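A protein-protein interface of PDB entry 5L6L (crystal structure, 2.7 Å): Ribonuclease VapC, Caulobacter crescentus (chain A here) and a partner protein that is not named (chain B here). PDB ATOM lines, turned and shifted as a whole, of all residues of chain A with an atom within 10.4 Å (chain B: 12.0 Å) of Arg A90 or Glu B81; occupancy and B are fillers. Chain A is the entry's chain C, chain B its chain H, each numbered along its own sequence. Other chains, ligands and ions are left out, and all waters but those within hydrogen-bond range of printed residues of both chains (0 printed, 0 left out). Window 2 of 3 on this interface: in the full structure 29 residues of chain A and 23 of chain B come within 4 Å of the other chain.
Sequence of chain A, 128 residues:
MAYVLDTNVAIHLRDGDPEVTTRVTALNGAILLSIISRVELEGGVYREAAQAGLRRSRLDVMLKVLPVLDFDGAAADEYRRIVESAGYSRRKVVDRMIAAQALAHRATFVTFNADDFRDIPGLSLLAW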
ATOM      1  N   TYR A  79       3.006 -34.687   2.180  1.00  0.00           N
ATOM      2  CA  TYR A  79       2.688 -33.592   3.084  1.00  0.00           C
ATOM      3  C   TYR A  79       3.831 -33.374   4.072  1.00  0.00           C
ATOM      4  O   TYR A  79       4.169 -32.228   4.392  1.00  0.00           O
ATOM      5  CB  TYR A  79       1.367 -33.847   3.810  1.00  0.00           C
ATOM      6  CG  TYR A  79       1.024 -32.787   4.861  1.00  0.00           C
ATOM      7  CD1 TYR A  79       0.223 -31.682   4.540  1.00  0.00           C
ATOM      8  CD2 TYR A  79       1.496 -32.896   6.172  1.00  0.00           C
ATOM      9  CE1 TYR A  79      -0.082 -30.719   5.486  1.00  0.00           C
ATOM     10  CE2 TYR A  79       1.205 -31.935   7.119  1.00  0.00           C
ATOM     11  CZ  TYR A  79       0.417 -30.850   6.774  1.00  0.00           C
ATOM     12  OH  TYR A  79       0.116 -29.906   7.715  1.00  0.00           O
ATOM     13  N   VAL A  83       5.799 -29.790   4.682  1.00  0.00           N
ATOM     14  CA  VAL A  83       5.891 -29.122   5.970  1.00  0.00           C
ATOM     15  C   VAL A  83       7.357 -28.949   6.394  1.00  0.00           C
ATOM     16  O   VAL A  83       7.725 -27.906   6.940  1.00  0.00           O
ATOM     17  CB  VAL A  83       5.004 -29.900   6.966  1.00  0.00           C
ATOM     18  CG1 VAL A  83       5.698 -30.319   8.187  1.00  0.00           C
ATOM     19  CG2 VAL A  83       3.782 -29.100   7.307  1.00  0.00           C
ATOM     20  N   ALA A  86       8.576 -25.761   4.144  1.00  0.00           N
ATOM     21  CA  ALA A  86       7.915 -24.473   4.213  1.00  0.00           C
ATOM     22  C   ALA A  86       7.442 -24.161   5.617  1.00  0.00           C
ATOM     23  O   ALA A  86       6.844 -23.099   5.837  1.00  0.00           O
ATOM     24  CB  ALA A  86       6.726 -24.438   3.243  1.00  0.00           C
ATOM     25  N   GLY A  87       7.697 -25.058   6.561  1.00  0.00           N
ATOM     26  CA  GLY A  87       7.220 -24.930   7.910  1.00  0.00           C
ATOM     27  C   GLY A  87       5.762 -25.329   8.031  1.00  0.00           C
ATOM     28  O   GLY A  87       5.027 -25.431   7.056  1.00  0.00           O
ATOM     29  N   TYR A  88       5.360 -25.567   9.274  1.00  0.00           N
ATOM     30  CA  TYR A  88       3.968 -25.804   9.603  1.00  0.00           C
ATOM     31  C   TYR A  88       3.134 -24.541   9.432  1.00  0.00           C
ATOM     32  O   TYR A  88       3.613 -23.418   9.626  1.00  0.00           O
ATOM     33  CB  TYR A  88       3.849 -26.288  11.038  1.00  0.00           C
ATOM     34  CG  TYR A  88       2.428 -26.474  11.486  1.00  0.00           C
ATOM     35  CD1 TYR A  88       1.638 -27.500  10.957  1.00  0.00           C
ATOM     36  CD2 TYR A  88       1.872 -25.637  12.441  1.00  0.00           C
ATOM     37  CE1 TYR A  88       0.342 -27.683  11.374  1.00  0.00           C
ATOM     38  CE2 TYR A  88       0.574 -25.814  12.871  1.00  0.00           C
ATOM     39  CZ  TYR A  88      -0.198 -26.837  12.332  1.00  0.00           C
ATOM     40  OH  TYR A  88      -1.506 -27.015  12.762  1.00  0.00           O
ATOM     41  N   SER A  89       1.864 -24.745   9.080  1.00  0.00           N
ATOM     42  CA  SER A  89       0.883 -23.664   8.998  1.00  0.00           C
ATOM     43  C   SER A  89      -0.509 -24.266   9.166  1.00  0.00           C
ATOM     44  O   SER A  89      -0.975 -24.995   8.280  1.00  0.00           O
ATOM     45  CB  SER A  89       1.000 -22.932   7.674  1.00  0.00           C
ATOM     46  OG  SER A  89      -0.188 -22.214   7.429  1.00  0.00           O
ATOM     47  N   ARG A  90      -1.181 -23.927  10.270  1.00  0.00           N
ATOM     48  CA  ARG A  90      -2.478 -24.534  10.570  1.00  0.00           C
ATOM     49  C   ARG A  90      -3.503 -24.273   9.472  1.00  0.00           C
ATOM     50  O   ARG A  90      -4.207 -25.188   9.048  1.00  0.00           O
ATOM     51  CB  ARG A  90      -3.021 -24.032  11.907  1.00  0.00           C
ATOM     52  CG  ARG A  90      -4.272 -24.815  12.300  1.00  0.00           C
ATOM     53  CD  ARG A  90      -4.551 -24.854  13.780  1.00  0.00           C
ATOM     54  NE  ARG A  90      -4.929 -23.537  14.258  1.00  0.00           N
ATOM     55  CZ  ARG A  90      -6.143 -23.014  14.148  1.00  0.00           C
ATOM     56  NH1 ARG A  90      -7.123 -23.706  13.566  1.00  0.00           N
ATOM     57  NH2 ARG A  90      -6.369 -21.790  14.621  1.00  0.00           N
ATOM     58  N   ARG A  91      -3.630 -23.027   9.023  1.00  0.00           N
ATOM     59  CA  ARG A  91      -4.688 -22.698   8.079  1.00  0.00           C
ATOM     60  C   ARG A  91      -4.419 -23.207   6.669  1.00  0.00           C
ATOM     61  O   ARG A  91      -5.344 -23.229   5.848  1.00  0.00           O
ATOM     62  CB  ARG A  91      -4.917 -21.190   8.042  1.00  0.00           C
ATOM     63  CG  ARG A  91      -4.448 -20.530   6.775  1.00  0.00           C
ATOM     64  CD  ARG A  91      -4.986 -19.135   6.671  1.00  0.00           C
ATOM     65  NE  ARG A  91      -5.960 -18.973   5.591  1.00  0.00           N
ATOM     66  CZ  ARG A  91      -7.260 -18.737   5.774  1.00  0.00           C
ATOM     67  NH1 ARG A  91      -7.761 -18.643   7.005  1.00  0.00           N
ATOM     68  NH2 ARG A  91      -8.060 -18.584   4.721  1.00  0.00           N
ATOM     69  N   LYS A  92      -3.202 -23.640   6.369  1.00  0.00           N
ATOM     70  CA  LYS A  92      -2.898 -24.199   5.067  1.00  0.00           C
ATOM     71  C   LYS A  92      -2.926 -25.736   5.021  1.00  0.00           C
ATOM     72  O   LYS A  92      -2.495 -26.304   4.019  1.00  0.00           O
ATOM     73  CB  LYS A  92      -1.537 -23.693   4.592  1.00  0.00           C
ATOM     74  CG  LYS A  92      -1.523 -22.257   4.112  1.00  0.00           C
ATOM     75  CD  LYS A  92      -0.280 -21.981   3.237  1.00  0.00           C
ATOM     76  CE  LYS A  92      -0.285 -20.573   2.624  1.00  0.00           C
ATOM     77  NZ  LYS A  92       0.954 -20.251   1.847  1.00  0.00           N
ATOM     78  N   VAL A  93      -3.439 -26.425   6.050  1.00  0.00           N
ATOM     79  CA  VAL A  93      -3.291 -27.886   6.091  1.00  0.00           C
ATOM     80  C   VAL A  93      -4.141 -28.554   5.013  1.00  0.00           C
ATOM     81  O   VAL A  93      -3.665 -29.436   4.292  1.00  0.00           O
ATOM     82  CB  VAL A  93      -3.622 -28.446   7.488  1.00  0.00           C
ATOM     83  CG1 VAL A  93      -3.568 -29.958   7.485  1.00  0.00           C
ATOM     84  CG2 VAL A  93      -2.656 -27.943   8.504  1.00  0.00           C
ATOM     85  N   VAL A  94      -5.406 -28.140   4.879  1.00  0.00           N
ATOM     86  CA  VAL A  94      -6.272 -28.682   3.834  1.00  0.00           C
ATOM     87  C   VAL A  94      -5.654 -28.481   2.454  1.00  0.00           C
ATOM     88  O   VAL A  94      -5.488 -29.437   1.689  1.00  0.00           O
ATOM     89  CB  VAL A  94      -7.669 -28.054   3.905  1.00  0.00           C
ATOM     90  CG1 VAL A  94      -8.482 -28.437   2.653  1.00  0.00           C
ATOM     91  CG2 VAL A  94      -8.382 -28.508   5.147  1.00  0.00           C
ATOM     92  N   ASP A  95      -5.329 -27.233   2.098  1.00  0.00           N
ATOM     93  CA  ASP A  95      -4.751 -27.004   0.772  1.00  0.00           C
ATOM     94  C   ASP A  95      -3.474 -27.814   0.564  1.00  0.00           C
ATOM     95  O   ASP A  95      -3.182 -28.239  -0.562  1.00  0.00           O
ATOM     96  CB  ASP A  95      -4.449 -25.521   0.540  1.00  0.00           C
ATOM     97  CG  ASP A  95      -5.659 -24.716   0.087  1.00  0.00           C
ATOM     98  OD1 ASP A  95      -6.685 -25.294  -0.316  1.00  0.00           O
ATOM     99  OD2 ASP A  95      -5.567 -23.469   0.116  1.00  0.00           O
ATOM    100  N   ARG A  96      -2.703 -28.041   1.624  1.00  0.00           N
ATOM    101  CA  ARG A  96      -1.454 -28.765   1.438  1.00  0.00           C
ATOM    102  C   ARG A  96      -1.676 -30.266   1.325  1.00  0.00           C
ATOM    103  O   ARG A  96      -0.847 -30.971   0.744  1.00  0.00           O
ATOM    104  CB  ARG A  96      -0.490 -28.461   2.578  1.00  0.00           C
ATOM    105  CG  ARG A  96       0.073 -27.086   2.513  1.00  0.00           C
ATOM    106  CD  ARG A  96       0.877 -26.769   3.729  1.00  0.00           C
ATOM    107  NE  ARG A  96       1.530 -25.466   3.653  1.00  0.00           N
ATOM    108  CZ  ARG A  96       2.360 -25.015   4.587  1.00  0.00           C
ATOM    109  NH1 ARG A  96       2.601 -25.772   5.651  1.00  0.00           N
ATOM    110  NH2 ARG A  96       2.942 -23.825   4.474  1.00  0.00           N
ATOM    111  N   MET A  97      -2.775 -30.770   1.862  1.00  0.00           N
ATOM    112  CA  MET A  97      -3.120 -32.172   1.677  1.00  0.00           C
ATOM    113  C   MET A  97      -3.500 -32.450   0.232  1.00  0.00           C
ATOM    114  O   MET A  97      -3.102 -33.448  -0.356  1.00  0.00           O
ATOM    115  CB  MET A  97      -4.255 -32.569   2.619  1.00  0.00           C
ATOM    116  CG  MET A  97      -3.832 -32.644   4.070  1.00  0.00           C
ATOM    117  SD  MET A  97      -5.273 -33.202   5.218  1.00  0.00           S
ATOM    118  CE  MET A  97      -5.415 -35.025   4.570  1.00  0.00           C
ATOM    119  N   ASP A 119       4.632 -21.964  -2.234  1.00  0.00           N
ATOM    120  CA  ASP A 119       5.608 -22.416  -1.249  1.00  0.00           C
ATOM    121  C   ASP A 119       5.731 -23.932  -1.200  1.00  0.00           C
ATOM    122  O   ASP A 119       6.498 -24.453  -0.380  1.00  0.00           O
ATOM    123  CB  ASP A 119       5.277 -21.861   0.152  1.00  0.00           C
ATOM    124  CG  ASP A 119       3.900 -22.294   0.675  1.00  0.00           C
ATOM    125  OD1 ASP A 119       3.056 -22.808  -0.093  1.00  0.00           O
ATOM    126  OD2 ASP A 119       3.663 -22.085   1.881  1.00  0.00           O
ATOM    127  N   ARG B  74     -16.090 -21.190   0.161  1.00  0.00           N
ATOM    128  CA  ARG B  74     -15.353 -22.230   0.865  1.00  0.00           C
ATOM    129  C   ARG B  74     -15.109 -21.856   2.317  1.00  0.00           C
ATOM    130  O   ARG B  74     -14.620 -20.765   2.611  1.00  0.00           O
ATOM    131  CB  ARG B  74     -14.018 -22.477   0.165  1.00  0.00           C
ATOM    132  CG  ARG B  74     -13.247 -23.647   0.714  1.00  0.00           C
ATOM    133  CD  ARG B  74     -11.868 -23.748   0.082  1.00  0.00           C
ATOM    134  NE  ARG B  74     -11.173 -24.948   0.526  1.00  0.00           N
ATOM    135  CZ  ARG B  74      -9.924 -25.251   0.201  1.00  0.00           C
ATOM    136  NH1 ARG B  74      -9.360 -26.372   0.645  1.00  0.00           N
ATOM    137  NH2 ARG B  74      -9.239 -24.443  -0.574  1.00  0.00           N
ATOM    138  N   ASP B  75     -15.485 -22.752   3.217  1.00  0.00           N
ATOM    139  CA  ASP B  75     -15.115 -22.617   4.622  1.00  0.00           C
ATOM    140  C   ASP B  75     -13.638 -22.937   4.800  1.00  0.00           C
ATOM    141  O   ASP B  75     -13.145 -23.946   4.287  1.00  0.00           O
ATOM    142  CB  ASP B  75     -15.951 -23.550   5.496  1.00  0.00           C
ATOM    143  CG  ASP B  75     -17.204 -22.900   6.026  1.00  0.00           C
ATOM    144  OD1 ASP B  75     -17.327 -21.656   5.951  1.00  0.00           O
ATOM    145  OD2 ASP B  75     -18.065 -23.641   6.542  1.00  0.00           O
ATOM    146  N   GLU B  76     -12.939 -22.092   5.540  1.00  0.00           N
ATOM    147  CA  GLU B  76     -11.513 -22.258   5.774  1.00  0.00           C
ATOM    148  C   GLU B  76     -11.272 -22.618   7.239  1.00  0.00           C
ATOM    149  O   GLU B  76     -12.209 -22.739   8.037  1.00  0.00           O
ATOM    150  CB  GLU B  76     -10.752 -20.998   5.343  1.00  0.00           C
ATOM    151  CG  GLU B  76      -9.856 -21.220   4.111  1.00  0.00           C
ATOM    152  CD  GLU B  76     -10.379 -20.568   2.828  1.00  0.00           C
ATOM    153  OE1 GLU B  76     -11.296 -19.726   2.894  1.00  0.00           O
ATOM    154  OE2 GLU B  76      -9.871 -20.896   1.732  1.00  0.00           O
ATOM    155  N   ASP B  77     -10.002 -22.846   7.577  1.00  0.00           N
ATOM    156  CA  ASP B  77      -9.569 -23.035   8.966  1.00  0.00           C
ATOM    157  C   ASP B  77     -10.088 -24.324   9.597  1.00  0.00           C
ATOM    158  O   ASP B  77     -10.267 -24.393  10.810  1.00  0.00           O
ATOM    159  CB  ASP B  77      -9.968 -21.847   9.826  1.00  0.00           C
ATOM    160  CG  ASP B  77      -8.996 -20.734   9.705  1.00  0.00           C
ATOM    161  OD1 ASP B  77      -7.797 -21.037   9.914  1.00  0.00           O
ATOM    162  OD2 ASP B  77      -9.412 -19.591   9.378  1.00  0.00           O
ATOM    163  N   LEU B  78     -10.265 -25.374   8.795  1.00  0.00           N
ATOM    164  CA  LEU B  78     -10.903 -26.587   9.285  1.00  0.00           C
ATOM    165  C   LEU B  78     -10.063 -27.307  10.340  1.00  0.00           C
ATOM    166  O   LEU B  78     -10.619 -27.863  11.297  1.00  0.00           O
ATOM    167  CB  LEU B  78     -11.208 -27.517   8.113  1.00  0.00           C
ATOM    168  CG  LEU B  78     -12.182 -27.015   7.055  1.00  0.00           C
ATOM    169  CD1 LEU B  78     -12.487 -28.148   6.081  1.00  0.00           C
ATOM    170  CD2 LEU B  78     -13.458 -26.426   7.656  1.00  0.00           C
ATOM    171  N   PHE B  79      -8.742 -27.336  10.192  1.00  0.00           N
ATOM    172  CA  PHE B  79      -7.920 -28.073  11.160  1.00  0.00           C
ATOM    173  C   PHE B  79      -7.787 -27.324  12.485  1.00  0.00           C
ATOM    174  O   PHE B  79      -7.276 -26.201  12.505  1.00  0.00           O
ATOM    175  CB  PHE B  79      -6.555 -28.377  10.560  1.00  0.00           C
ATOM    176  CG  PHE B  79      -6.543 -29.648   9.852  1.00  0.00           C
ATOM    177  CD1 PHE B  79      -6.317 -30.828  10.548  1.00  0.00           C
ATOM    178  CD2 PHE B  79      -6.897 -29.709   8.507  1.00  0.00           C
ATOM    179  CE1 PHE B  79      -6.386 -32.053   9.910  1.00  0.00           C
ATOM    180  CE2 PHE B  79      -6.962 -30.931   7.846  1.00  0.00           C
ATOM    181  CZ  PHE B  79      -6.707 -32.110   8.551  1.00  0.00           C
ATOM    182  N   PRO B  80      -8.220 -27.896  13.601  1.00  0.00           N
ATOM    183  CA  PRO B  80      -8.251 -27.144  14.862  1.00  0.00           C
ATOM    184  C   PRO B  80      -6.889 -27.047  15.530  1.00  0.00           C
ATOM    185  O   PRO B  80      -5.957 -27.798  15.238  1.00  0.00           O
ATOM    186  CB  PRO B  80      -9.203 -27.973  15.729  1.00  0.00           C
ATOM    187  CG  PRO B  80      -8.970 -29.371  15.262  1.00  0.00           C
ATOM    188  CD  PRO B  80      -8.728 -29.273  13.764  1.00  0.00           C
ATOM    189  N   GLU B  81      -6.787 -26.093  16.450  1.00  0.00           N
ATOM    190  CA  GLU B  81      -5.712 -26.147  17.439  1.00  0.00           C
ATOM    191  C   GLU B  81      -5.938 -27.339  18.351  1.00  0.00           C
ATOM    192  O   GLU B  81      -7.019 -27.513  18.919  1.00  0.00           O
ATOM    193  CB  GLU B  81      -5.653 -24.890  18.300  1.00  0.00           C
ATOM    194  CG  GLU B  81      -5.398 -23.594  17.573  1.00  0.00           C
ATOM    195  CD  GLU B  81      -5.856 -22.385  18.387  1.00  0.00           C
ATOM    196  OE1 GLU B  81      -6.022 -22.514  19.631  1.00  0.00           O
ATOM    197  OE2 GLU B  81      -6.064 -21.314  17.771  1.00  0.00           O
ATOM    198  N   ARG B  82      -4.920 -28.160  18.495  1.00  0.00           N
ATOM    199  CA  ARG B  82      -4.984 -29.210  19.457  1.00  0.00           C
ATOM    200  C   ARG B  82      -3.855 -28.994  20.443  1.00  0.00           C
ATOM    201  O   ARG B  82      -2.736 -28.670  20.020  1.00  0.00           O
ATOM    202  CB  ARG B  82      -4.852 -30.577  18.777  1.00  0.00           C
ATOM    203  CG  ARG B  82      -5.846 -30.750  17.680  1.00  0.00           C
ATOM    204  CD  ARG B  82      -6.315 -32.147  17.662  1.00  0.00           C
ATOM    205  NE  ARG B  82      -6.810 -32.520  16.350  1.00  0.00           N
ATOM    206  CZ  ARG B  82      -8.072 -32.786  16.093  1.00  0.00           C
ATOM    207  NH1 ARG B  82      -8.422 -33.117  14.866  1.00  0.00           N
ATOM    208  NH2 ARG B  82      -8.974 -32.706  17.049  1.00  0.00           N
ATOM    209  N   PRO B  83      -4.100 -29.119  21.743  1.00  0.00           N
ATOM    210  CA  PRO B  83      -2.992 -29.001  22.706  1.00  0.00           C
ATOM    211  C   PRO B  83      -1.891 -30.013  22.404  1.00  0.00           C
ATOM    212  O   PRO B  83      -2.156 -31.194  22.164  1.00  0.00           O
ATOM    213  CB  PRO B  83      -3.661 -29.263  24.064  1.00  0.00           C
ATOM    214  CG  PRO B  83      -5.160 -29.290  23.798  1.00  0.00           C
ATOM    215  CD  PRO B  83      -5.425 -28.983  22.370  1.00  0.00           C
ATOM    216  N   GLY B  84      -0.649 -29.531  22.378  1.00  0.00           N
ATOM    217  CA  GLY B  84       0.498 -30.397  22.138  1.00  0.00           C
ATOM    218  C   GLY B  84       1.024 -30.417  20.709  1.00  0.00           C
ATOM    219  O   GLY B  84       0.267 -30.353  19.733  1.00  0.00           O
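Among the printed residues, pairs that only touch across the chains: Arg A90 with Pro B80 (3.6 Å), Val A93 with Phe B79 (3.5 Å), Val A94 with Arg B74 (3.0 Å), Val A94 with Phe B79 (3.9 Å) and Met A97 with Phe B79 (3.8 Å).
Of the 15 printed residues of chain A, 6 touch a printed residue of chain B. Printed residues of chain A that touch a printed residue of chain B: Arg A90, Arg A91, Val A93, Val A94, Asp A95 and Met A97. Hydrophobic or aromatic side chains of chain A that line the printed part of chain B: Val A93, Val A94 and Met A97. Among the printed residues, 10 pairs touch across the chains. Among the printed residues, Asp or Glu carboxylates within 4 Å of a Lys or Arg side-chain nitrogen of the other chain: Arg A90 with Glu B81, Arg A91 with Glu B76, Arg A91 with Asp B77 and Asp A95 with Arg B74.
The guanidinium group of Arg A90 is in salt-bridge range of the side-chain carboxylate of Glu B81 (3.2 Å). The guanidinium group (NH2) of Arg B74 is in salt-bridge range of the side-chain carboxylate (OD1) of Asp A95 (2.7 Å). The guanidinium group of Arg A91 is in salt-bridge range of the side-chain carboxylate of Glu B76 (3.9 Å). The side-chain carboxylate of Asp B77 is in salt-bridge range of the guanidinium group of Arg A91 (3.0 Å). O of Phe B79 is in hydrogen-bond range of NH1 of Arg A90, at 2.7 Å.
Of chain B, only Phe B79, Pro B80 and Glu B81 come within 4 Å of Arg A90. Glu B81 touches just one residue of chain A: Arg A90. Tyr A88 touches none of the printed residues of chain B. No residue of chain B comes within 4 Å of Ser A89. Val A93 touches just one residue of chain B: Phe B79. Printed residues of chain A within 4 Å of Glu B76: Arg A91 (3.2 Å). Of the printed residues of chain A, Asp B77 touches Arg A91.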
